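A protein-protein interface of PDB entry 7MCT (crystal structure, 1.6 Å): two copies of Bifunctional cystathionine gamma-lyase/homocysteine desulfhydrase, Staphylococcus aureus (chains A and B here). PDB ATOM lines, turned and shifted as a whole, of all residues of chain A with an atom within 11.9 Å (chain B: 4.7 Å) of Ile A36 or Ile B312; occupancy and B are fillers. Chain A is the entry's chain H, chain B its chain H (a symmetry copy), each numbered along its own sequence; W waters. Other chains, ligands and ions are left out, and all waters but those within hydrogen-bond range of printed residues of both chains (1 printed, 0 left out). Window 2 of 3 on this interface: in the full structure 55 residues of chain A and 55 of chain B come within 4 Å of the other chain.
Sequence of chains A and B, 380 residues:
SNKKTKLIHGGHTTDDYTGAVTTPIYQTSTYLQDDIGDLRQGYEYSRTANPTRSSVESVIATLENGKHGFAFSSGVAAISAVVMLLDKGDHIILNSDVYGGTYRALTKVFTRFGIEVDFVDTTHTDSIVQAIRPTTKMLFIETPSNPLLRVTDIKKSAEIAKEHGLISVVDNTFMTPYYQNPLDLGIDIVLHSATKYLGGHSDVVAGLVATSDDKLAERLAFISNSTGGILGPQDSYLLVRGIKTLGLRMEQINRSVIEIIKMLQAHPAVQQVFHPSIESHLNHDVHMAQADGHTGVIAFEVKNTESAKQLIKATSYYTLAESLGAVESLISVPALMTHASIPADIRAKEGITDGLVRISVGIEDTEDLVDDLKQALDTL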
ATOM      1  N   TYR A  31     -19.384  -0.724  26.099  1.00  0.00           N
ATOM      2  CA  TYR A  31     -20.839  -0.807  26.048  1.00  0.00           C
ATOM      3  C   TYR A  31     -21.342  -0.478  24.650  1.00  0.00           C
ATOM      4  O   TYR A  31     -20.868   0.470  24.014  1.00  0.00           O
ATOM      5  CB  TYR A  31     -21.484   0.145  27.078  1.00  0.00           C
ATOM      6  CG  TYR A  31     -20.961  -0.078  28.483  1.00  0.00           C
ATOM      7  CD1 TYR A  31     -19.736   0.456  28.883  1.00  0.00           C
ATOM      8  CD2 TYR A  31     -21.676  -0.831  29.399  1.00  0.00           C
ATOM      9  CE1 TYR A  31     -19.238   0.231  30.144  1.00  0.00           C
ATOM     10  CE2 TYR A  31     -21.186  -1.059  30.674  1.00  0.00           C
ATOM     11  CZ  TYR A  31     -19.962  -0.516  31.036  1.00  0.00           C
ATOM     12  OH  TYR A  31     -19.476  -0.751  32.297  1.00  0.00           O
ATOM     13  N   LEU A  32     -22.315  -1.263  24.188  1.00  0.00           N
ATOM     14  CA  LEU A  32     -22.949  -1.010  22.901  1.00  0.00           C
ATOM     15  C   LEU A  32     -23.620   0.352  22.889  1.00  0.00           C
ATOM     16  O   LEU A  32     -24.247   0.761  23.874  1.00  0.00           O
ATOM     17  CB  LEU A  32     -24.006  -2.073  22.615  1.00  0.00           C
ATOM     18  CG  LEU A  32     -23.583  -3.534  22.677  1.00  0.00           C
ATOM     19  CD1 LEU A  32     -24.795  -4.455  22.712  1.00  0.00           C
ATOM     20  CD2 LEU A  32     -22.746  -3.824  21.479  1.00  0.00           C
ATOM     21  N   GLN A  33     -23.495   1.053  21.765  1.00  0.00           N
ATOM     22  CA  GLN A  33     -24.247   2.275  21.513  1.00  0.00           C
ATOM     23  C   GLN A  33     -25.214   2.010  20.366  1.00  0.00           C
ATOM     24  O   GLN A  33     -24.819   1.465  19.328  1.00  0.00           O
ATOM     25  CB  GLN A  33     -23.316   3.447  21.183  1.00  0.00           C
ATOM     26  CG  GLN A  33     -22.322   3.741  22.302  1.00  0.00           C
ATOM     27  CD  GLN A  33     -21.373   4.874  21.972  1.00  0.00           C
ATOM     28  OE1 GLN A  33     -21.679   5.749  21.158  1.00  0.00           O
ATOM     29  NE2 GLN A  33     -20.203   4.861  22.604  1.00  0.00           N
ATOM     30  N   ASP A  34     -26.485   2.355  20.571  1.00  0.00           N
ATOM     31  CA  ASP A  34     -27.483   2.108  19.534  1.00  0.00           C
ATOM     32  C   ASP A  34     -27.378   3.135  18.416  1.00  0.00           C
ATOM     33  O   ASP A  34     -27.660   2.824  17.254  1.00  0.00           O
ATOM     34  CB  ASP A  34     -28.881   2.110  20.152  1.00  0.00           C
ATOM     35  CG  ASP A  34     -29.083   0.955  21.112  1.00  0.00           C
ATOM     36  OD1 ASP A  34     -28.604  -0.155  20.795  1.00  0.00           O
ATOM     37  OD2 ASP A  34     -29.685   1.156  22.187  1.00  0.00           O
ATOM     38  N   ASP A  35     -26.977   4.352  18.755  1.00  0.00           N
ATOM     39  CA  ASP A  35     -26.618   5.386  17.800  1.00  0.00           C
ATOM     40  C   ASP A  35     -25.396   6.083  18.363  1.00  0.00           C
ATOM     41  O   ASP A  35     -25.180   6.071  19.576  1.00  0.00           O
ATOM     42  CB  ASP A  35     -27.754   6.394  17.586  1.00  0.00           C
ATOM     43  CG  ASP A  35     -28.961   5.774  16.915  1.00  0.00           C
ATOM     44  OD1 ASP A  35     -28.909   5.548  15.688  1.00  0.00           O
ATOM     45  OD2 ASP A  35     -29.955   5.497  17.621  1.00  0.00           O
ATOM     46  N   ILE A  36     -24.593   6.685  17.484  1.00  0.00           N
ATOM     47  CA  ILE A  36     -23.382   7.357  17.950  1.00  0.00           C
ATOM     48  C   ILE A  36     -23.770   8.420  18.964  1.00  0.00           C
ATOM     49  O   ILE A  36     -24.535   9.341  18.657  1.00  0.00           O
ATOM     50  CB  ILE A  36     -22.600   7.955  16.777  1.00  0.00           C
ATOM     51  CG1 ILE A  36     -22.053   6.849  15.878  1.00  0.00           C
ATOM     52  CG2 ILE A  36     -21.461   8.822  17.288  1.00  0.00           C
ATOM     53  CD1 ILE A  36     -21.296   7.367  14.678  1.00  0.00           C
ATOM     54  N   GLY A  37     -23.265   8.277  20.192  1.00  0.00           N
ATOM     55  CA  GLY A  37     -23.513   9.218  21.259  1.00  0.00           C
ATOM     56  C   GLY A  37     -24.673   8.862  22.167  1.00  0.00           C
ATOM     57  O   GLY A  37     -24.794   9.447  23.251  1.00  0.00           O
ATOM     58  N   ASP A  38     -25.528   7.929  21.760  1.00  0.00           N
ATOM     59  CA  ASP A  38     -26.674   7.524  22.566  1.00  0.00           C
ATOM     60  C   ASP A  38     -26.264   6.343  23.438  1.00  0.00           C
ATOM     61  O   ASP A  38     -26.034   5.237  22.936  1.00  0.00           O
ATOM     62  CB  ASP A  38     -27.866   7.167  21.681  1.00  0.00           C
ATOM     63  CG  ASP A  38     -28.503   8.386  21.036  1.00  0.00           C
ATOM     64  OD2 ASP A  38     -27.980   9.505  21.234  1.00  0.00           O
ATOM     65  N   LEU A  39     -26.180   6.578  24.744  1.00  0.00           N
ATOM     66  CA  LEU A  39     -25.873   5.539  25.717  1.00  0.00           C
ATOM     67  C   LEU A  39     -27.174   5.005  26.303  1.00  0.00           C
ATOM     68  O   LEU A  39     -28.026   5.785  26.737  1.00  0.00           O
ATOM     69  CB  LEU A  39     -24.966   6.087  26.822  1.00  0.00           C
ATOM     70  CG  LEU A  39     -23.771   6.917  26.338  1.00  0.00           C
ATOM     71  CD1 LEU A  39     -22.941   7.434  27.509  1.00  0.00           C
ATOM     72  CD2 LEU A  39     -22.910   6.100  25.382  1.00  0.00           C
ATOM     73  N   ARG A  40     -27.324   3.677  26.314  1.00  0.00           N
ATOM     74  CA  ARG A  40     -28.568   3.070  26.784  1.00  0.00           C
ATOM     75  C   ARG A  40     -28.886   3.481  28.214  1.00  0.00           C
ATOM     76  O   ARG A  40     -30.032   3.815  28.537  1.00  0.00           O
ATOM     77  CB  ARG A  40     -28.482   1.546  26.701  1.00  0.00           C
ATOM     78  CG  ARG A  40     -28.362   1.015  25.307  1.00  0.00           C
ATOM     79  CD  ARG A  40     -28.497  -0.492  25.290  1.00  0.00           C
ATOM     80  NE  ARG A  40     -28.373  -0.970  23.923  1.00  0.00           N
ATOM     81  CZ  ARG A  40     -28.222  -2.244  23.591  1.00  0.00           C
ATOM     82  NH1 ARG A  40     -28.175  -3.171  24.537  1.00  0.00           N
ATOM     83  NH2 ARG A  40     -28.114  -2.583  22.313  1.00  0.00           N
ATOM     84  N   TYR A  43     -23.700   4.444  30.283  1.00  0.00           N
ATOM     85  CA  TYR A  43     -22.385   3.818  30.320  1.00  0.00           C
ATOM     86  C   TYR A  43     -21.782   3.773  28.924  1.00  0.00           C
ATOM     87  O   TYR A  43     -22.480   3.512  27.938  1.00  0.00           O
ATOM     88  CB  TYR A  43     -22.473   2.406  30.928  1.00  0.00           C
ATOM     89  CG  TYR A  43     -22.872   2.508  32.377  1.00  0.00           C
ATOM     90  CD1 TYR A  43     -21.918   2.773  33.353  1.00  0.00           C
ATOM     91  CD2 TYR A  43     -24.204   2.423  32.766  1.00  0.00           C
ATOM     92  CE1 TYR A  43     -22.275   2.916  34.680  1.00  0.00           C
ATOM     93  CE2 TYR A  43     -24.571   2.572  34.098  1.00  0.00           C
ATOM     94  CZ  TYR A  43     -23.594   2.825  35.047  1.00  0.00           C
ATOM     95  OH  TYR A  43     -23.931   2.980  36.371  1.00  0.00           O
ATOM     96  N   GLU A  44     -20.482   4.048  28.849  1.00  0.00           N
ATOM     97  CA  GLU A  44     -19.770   4.014  27.575  1.00  0.00           C
ATOM     98  C   GLU A  44     -18.377   3.405  27.662  1.00  0.00           C
ATOM     99  O   GLU A  44     -17.931   2.819  26.669  1.00  0.00           O
ATOM    100  CB  GLU A  44     -19.699   5.428  26.968  1.00  0.00           C
ATOM    101  CG  GLU A  44     -18.432   6.198  27.165  1.00  0.00           C
ATOM    102  CD  GLU A  44     -18.552   7.628  26.626  1.00  0.00           C
ATOM    103  OE1 GLU A  44     -18.863   8.533  27.423  1.00  0.00           O
ATOM    104  OE2 GLU A  44     -18.349   7.836  25.409  1.00  0.00           O
ATOM    105  N   ALA B 308     -20.745   7.577   6.850  1.00  0.00           N
ATOM    106  CA  ALA B 308     -20.182   6.826   7.970  1.00  0.00           C
ATOM    107  C   ALA B 308     -21.284   6.184   8.810  1.00  0.00           C
ATOM    108  O   ALA B 308     -21.200   5.001   9.175  1.00  0.00           O
ATOM    109  CB  ALA B 308     -19.305   7.747   8.824  1.00  0.00           C
ATOM    110  N   LYS B 309     -22.333   6.953   9.124  1.00  0.00           N
ATOM    111  CA  LYS B 309     -23.439   6.403   9.905  1.00  0.00           C
ATOM    112  C   LYS B 309     -24.138   5.275   9.156  1.00  0.00           C
ATOM    113  O   LYS B 309     -24.487   4.245   9.754  1.00  0.00           O
ATOM    114  CB  LYS B 309     -24.434   7.506  10.268  1.00  0.00           C
ATOM    115  CG  LYS B 309     -23.923   8.468  11.329  1.00  0.00           C
ATOM    116  CD  LYS B 309     -24.957   9.524  11.668  1.00  0.00           C
ATOM    117  CE  LYS B 309     -24.514  10.360  12.859  1.00  0.00           C
ATOM    118  NZ  LYS B 309     -25.484  11.445  13.165  1.00  0.00           N
ATOM    119  N   GLN B 310     -24.340   5.446   7.846  1.00  0.00           N
ATOM    120  CA  GLN B 310     -24.980   4.396   7.055  1.00  0.00           C
ATOM    121  C   GLN B 310     -24.127   3.136   7.022  1.00  0.00           C
ATOM    122  O   GLN B 310     -24.653   2.016   7.106  1.00  0.00           O
ATOM    123  CB  GLN B 310     -25.244   4.905   5.635  1.00  0.00           C
ATOM    124  CG  GLN B 310     -25.691   3.831   4.643  1.00  0.00           C
ATOM    125  CD  GLN B 310     -26.926   3.069   5.101  1.00  0.00           C
ATOM    126  OE1 GLN B 310     -27.769   3.601   5.826  1.00  0.00           O
ATOM    127  NE2 GLN B 310     -27.037   1.812   4.673  1.00  0.00           N
ATOM    128  N   LEU B 311     -22.811   3.297   6.886  1.00  0.00           N
ATOM    129  CA  LEU B 311     -21.895   2.165   6.948  1.00  0.00           C
ATOM    130  C   LEU B 311     -22.071   1.396   8.251  1.00  0.00           C
ATOM    131  O   LEU B 311     -22.189   0.163   8.252  1.00  0.00           O
ATOM    132  CB  LEU B 311     -20.455   2.675   6.807  1.00  0.00           C
ATOM    133  CG  LEU B 311     -19.368   1.606   6.744  1.00  0.00           C
ATOM    134  CD1 LEU B 311     -19.554   0.753   5.498  1.00  0.00           C
ATOM    135  CD2 LEU B 311     -17.984   2.244   6.768  1.00  0.00           C
ATOM    136  N   ILE B 312     -22.107   2.117   9.372  1.00  0.00           N
ATOM    137  CA  ILE B 312     -22.263   1.458  10.668  1.00  0.00           C
ATOM    138  C   ILE B 312     -23.587   0.700  10.732  1.00  0.00           C
ATOM    139  O   ILE B 312     -23.650  -0.429  11.239  1.00  0.00           O
ATOM    140  CB  ILE B 312     -22.149   2.483  11.808  1.00  0.00           C
ATOM    141  CG1 ILE B 312     -20.715   2.994  11.908  1.00  0.00           C
ATOM    142  CG2 ILE B 312     -22.593   1.874  13.128  1.00  0.00           C
ATOM    143  CD1 ILE B 312     -20.578   4.218  12.788  1.00  0.00           C
ATOM    144  N   LYS B 313     -24.663   1.305  10.226  1.00  0.00           N
ATOM    145  CA  LYS B 313     -25.968   0.650  10.334  1.00  0.00           C
ATOM    146  C   LYS B 313     -26.101  -0.538   9.386  1.00  0.00           C
ATOM    147  O   LYS B 313     -26.876  -1.464   9.663  1.00  0.00           O
ATOM    148  CB  LYS B 313     -27.090   1.655  10.079  1.00  0.00           C
ATOM    149  CG  LYS B 313     -27.201   2.739  11.142  1.00  0.00           C
ATOM    150  CD  LYS B 313     -28.259   2.394  12.186  1.00  0.00           C
ATOM    151  CE  LYS B 313     -28.564   3.586  13.087  1.00  0.00           C
ATOM    152  NZ  LYS B 313     -28.440   3.245  14.535  1.00  0.00           N
ATOM    153  N   ALA B 314     -25.362  -0.540   8.276  1.00  0.00           N
ATOM    154  CA  ALA B 314     -25.521  -1.584   7.270  1.00  0.00           C
ATOM    155  C   ALA B 314     -24.703  -2.838   7.563  1.00  0.00           C
ATOM    156  O   ALA B 314     -24.998  -3.892   6.991  1.00  0.00           O
ATOM    157  CB  ALA B 314     -25.144  -1.045   5.889  1.00  0.00           C
ATOM    158  N   THR B 315     -23.688  -2.755   8.421  1.00  0.00           N
ATOM    159  CA  THR B 315     -22.884  -3.926   8.738  1.00  0.00           C
ATOM    160  C   THR B 315     -23.643  -4.847   9.687  1.00  0.00           C
ATOM    161  O   THR B 315     -24.453  -4.402  10.503  1.00  0.00           O
ATOM    162  CB  THR B 315     -21.550  -3.522   9.377  1.00  0.00           C
ATOM    163  OG1 THR B 315     -21.788  -2.604  10.450  1.00  0.00           O
ATOM    164  CG2 THR B 315     -20.639  -2.858   8.360  1.00  0.00           C
ATOM    165  N   LEU B 320     -20.756  -1.058  17.119  1.00  0.00           N
ATOM    166  CA  LEU B 320     -20.499   0.329  17.502  1.00  0.00           C
ATOM    167  C   LEU B 320     -20.269   0.394  19.007  1.00  0.00           C
ATOM    168  O   LEU B 320     -21.199   0.192  19.796  1.00  0.00           O
ATOM    169  CB  LEU B 320     -21.667   1.218  17.087  1.00  0.00           C
ATOM    170  CG  LEU B 320     -21.577   2.693  17.459  1.00  0.00           C
ATOM    171  CD1 LEU B 320     -20.340   3.334  16.836  1.00  0.00           C
ATOM    172  CD2 LEU B 320     -22.848   3.415  17.032  1.00  0.00           C
ATOM    173  N   ILE B 331     -16.398  -0.711  15.472  1.00  0.00           N
ATOM    174  CA  ILE B 331     -16.396   0.370  14.494  1.00  0.00           C
ATOM    175  C   ILE B 331     -16.747   1.663  15.210  1.00  0.00           C
ATOM    176  O   ILE B 331     -17.510   1.669  16.182  1.00  0.00           O
ATOM    177  CB  ILE B 331     -17.381   0.070  13.335  1.00  0.00           C
ATOM    178  CG1 ILE B 331     -17.291   1.121  12.222  1.00  0.00           C
ATOM    179  CG2 ILE B 331     -18.797  -0.045  13.859  1.00  0.00           C
ATOM    180  CD1 ILE B 331     -17.695   0.566  10.849  1.00  0.00           C
ATOM    181  N   VAL B 333     -16.438   6.383  14.725  1.00  0.00           N
ATOM    182  CA  VAL B 333     -16.205   7.577  13.911  1.00  0.00           C
ATOM    183  C   VAL B 333     -15.480   8.594  14.785  1.00  0.00           C
ATOM    184  O   VAL B 333     -16.122   9.279  15.594  1.00  0.00           O
ATOM    185  CB  VAL B 333     -17.521   8.152  13.358  1.00  0.00           C
ATOM    186  CG1 VAL B 333     -17.252   9.391  12.496  1.00  0.00           C
ATOM    187  CG2 VAL B 333     -18.270   7.098  12.553  1.00  0.00           C
ATOM    188  N   LEU B 336     -16.851  12.155  15.624  1.00  0.00           N
ATOM    189  CA  LEU B 336     -18.039  12.238  16.462  1.00  0.00           C
ATOM    190  C   LEU B 336     -17.834  11.695  17.870  1.00  0.00           C
ATOM    191  O   LEU B 336     -18.591  12.065  18.774  1.00  0.00           O
ATOM    192  CB  LEU B 336     -19.201  11.479  15.807  1.00  0.00           C
ATOM    193  CG  LEU B 336     -19.693  12.017  14.463  1.00  0.00           C
ATOM    194  CD1 LEU B 336     -20.646  11.039  13.804  1.00  0.00           C
ATOM    195  CD2 LEU B 336     -20.364  13.367  14.654  1.00  0.00           C
ATOM    196  N   MET B 337     -16.845  10.834  18.085  1.00  0.00           N
ATOM    197  CA  MET B 337     -16.765  10.082  19.331  1.00  0.00           C
ATOM    198  C   MET B 337     -15.552  10.435  20.176  1.00  0.00           C
ATOM    199  O   MET B 337     -15.688  10.670  21.380  1.00  0.00           O
ATOM    200  CB  MET B 337     -16.779   8.576  19.028  1.00  0.00           C
ATOM    201  CG  MET B 337     -18.116   8.119  18.482  1.00  0.00           C
ATOM    202  SD  MET B 337     -18.158   6.441  17.823  1.00  0.00           S
ATOM    203  CE  MET B 337     -17.748   5.462  19.273  1.00  0.00           C
HETATM  204  O   HOH W   1     -25.810   2.790  14.643  1.00  0.00           O
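The backbone carbonyl oxygen (O) of Asp A34 sits at hydrogen-bond distance from the side-chain amino group (NZ) of Lys B313 (2.9 Å). The backbone NH (N) of Gln A33 lies within hydrogen-bond range of the backbone carbonyl oxygen (O) of Leu B320. OD1 of Asp A35 is in salt-bridge range of NZ of Lys B313, at 2.6 Å.
O of Ile B312 is in hydrogen-bond range of OG1 of Thr B315 (3.0 Å). N of Gly A37 sits at hydrogen-bond distance from OE1 of Gln A33 (3.1 Å). The side-chain carboxylate of Asp A34 lies within salt-bridge range of the guanidinium group of Arg A40 (2.9 Å). The side-chain sulfur of Met B337 lies within hydrogen-bond range of the backbone NH of Val B333 (3.5 Å).
Among the printed residues, pairs that only touch across the chains: Leu A32 with Leu B320, Asp A35 with Leu B320, Ile A36 with Ile B312, Ile A36 with Leu B320, Ile A36 with Val B333, Ile A36 with Leu B336 and Ile A36 with Met B337.
Ile A36 touches five residues of chain B. Ile B312 touches just one residue of chain A: Ile A36. No residue of chain A comes within 4 Å of Ala B308. Lys B309 touches none of the printed residues of chain A. Gln B310 touches none of the printed residues of chain A. Lys B313 touches just these residues of chain A: Asp A34 (2.9 Å) and Asp A35 (2.6 Å). No residue of chain A comes within 4 Å of Ala B314. No residue of chain A comes within 4 Å of Thr B315. Of chain A, only Leu A32, Gln A33, Asp A35 and Ile A36 come within 4 Å of Leu B320. Ile B331 touches none of the printed residues of chain A. Of the printed residues of chain A, Val B333 touches Ile A36. Of chain A, only Ile A36 comes within 4 Å of Leu B336. Of the printed residues of chain B, Gln A33 touches Leu B320. Of the printed residues of chain B, Asp A35 touches Lys B313 and Leu B320. Printed residues of chain B within 4 Å of Asp A34: Lys B313 (2.9 Å). Of the printed residues of chain B, Leu A32 touches Leu B320. Asp A38 touches none of the printed residues of chain B. The nearest residue of chain B that does not touch Ile A36 is Lys B309 (4.4 Å). The nearest printed residue of chain A that does not touch Ile B312 is Gln A33 (6.6 Å).
Printed residues of chain A that touch a printed residue of chain B: Leu A32, Gln A33, Asp A34, Asp A35 and Ile A36. Hydrophobic or aromatic side chains of chain A that line the printed part of chain B: Ile A36. Along chain A the printed residues that touch a printed residue of chain B span positions 32 to 36. Among the printed residues, 10 pairs touch across the chains.
No position is printed for both chains. Of the 10 pairs that touch across the chains among the printed residues, none has its exchanged pair printed and touching as well.
Water W1 lies within hydrogen-bond range of the side-chain amino group of Lys B313 (2.7 Å) and the backbone carbonyl oxygen of Asp A34 (3.2 Å).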
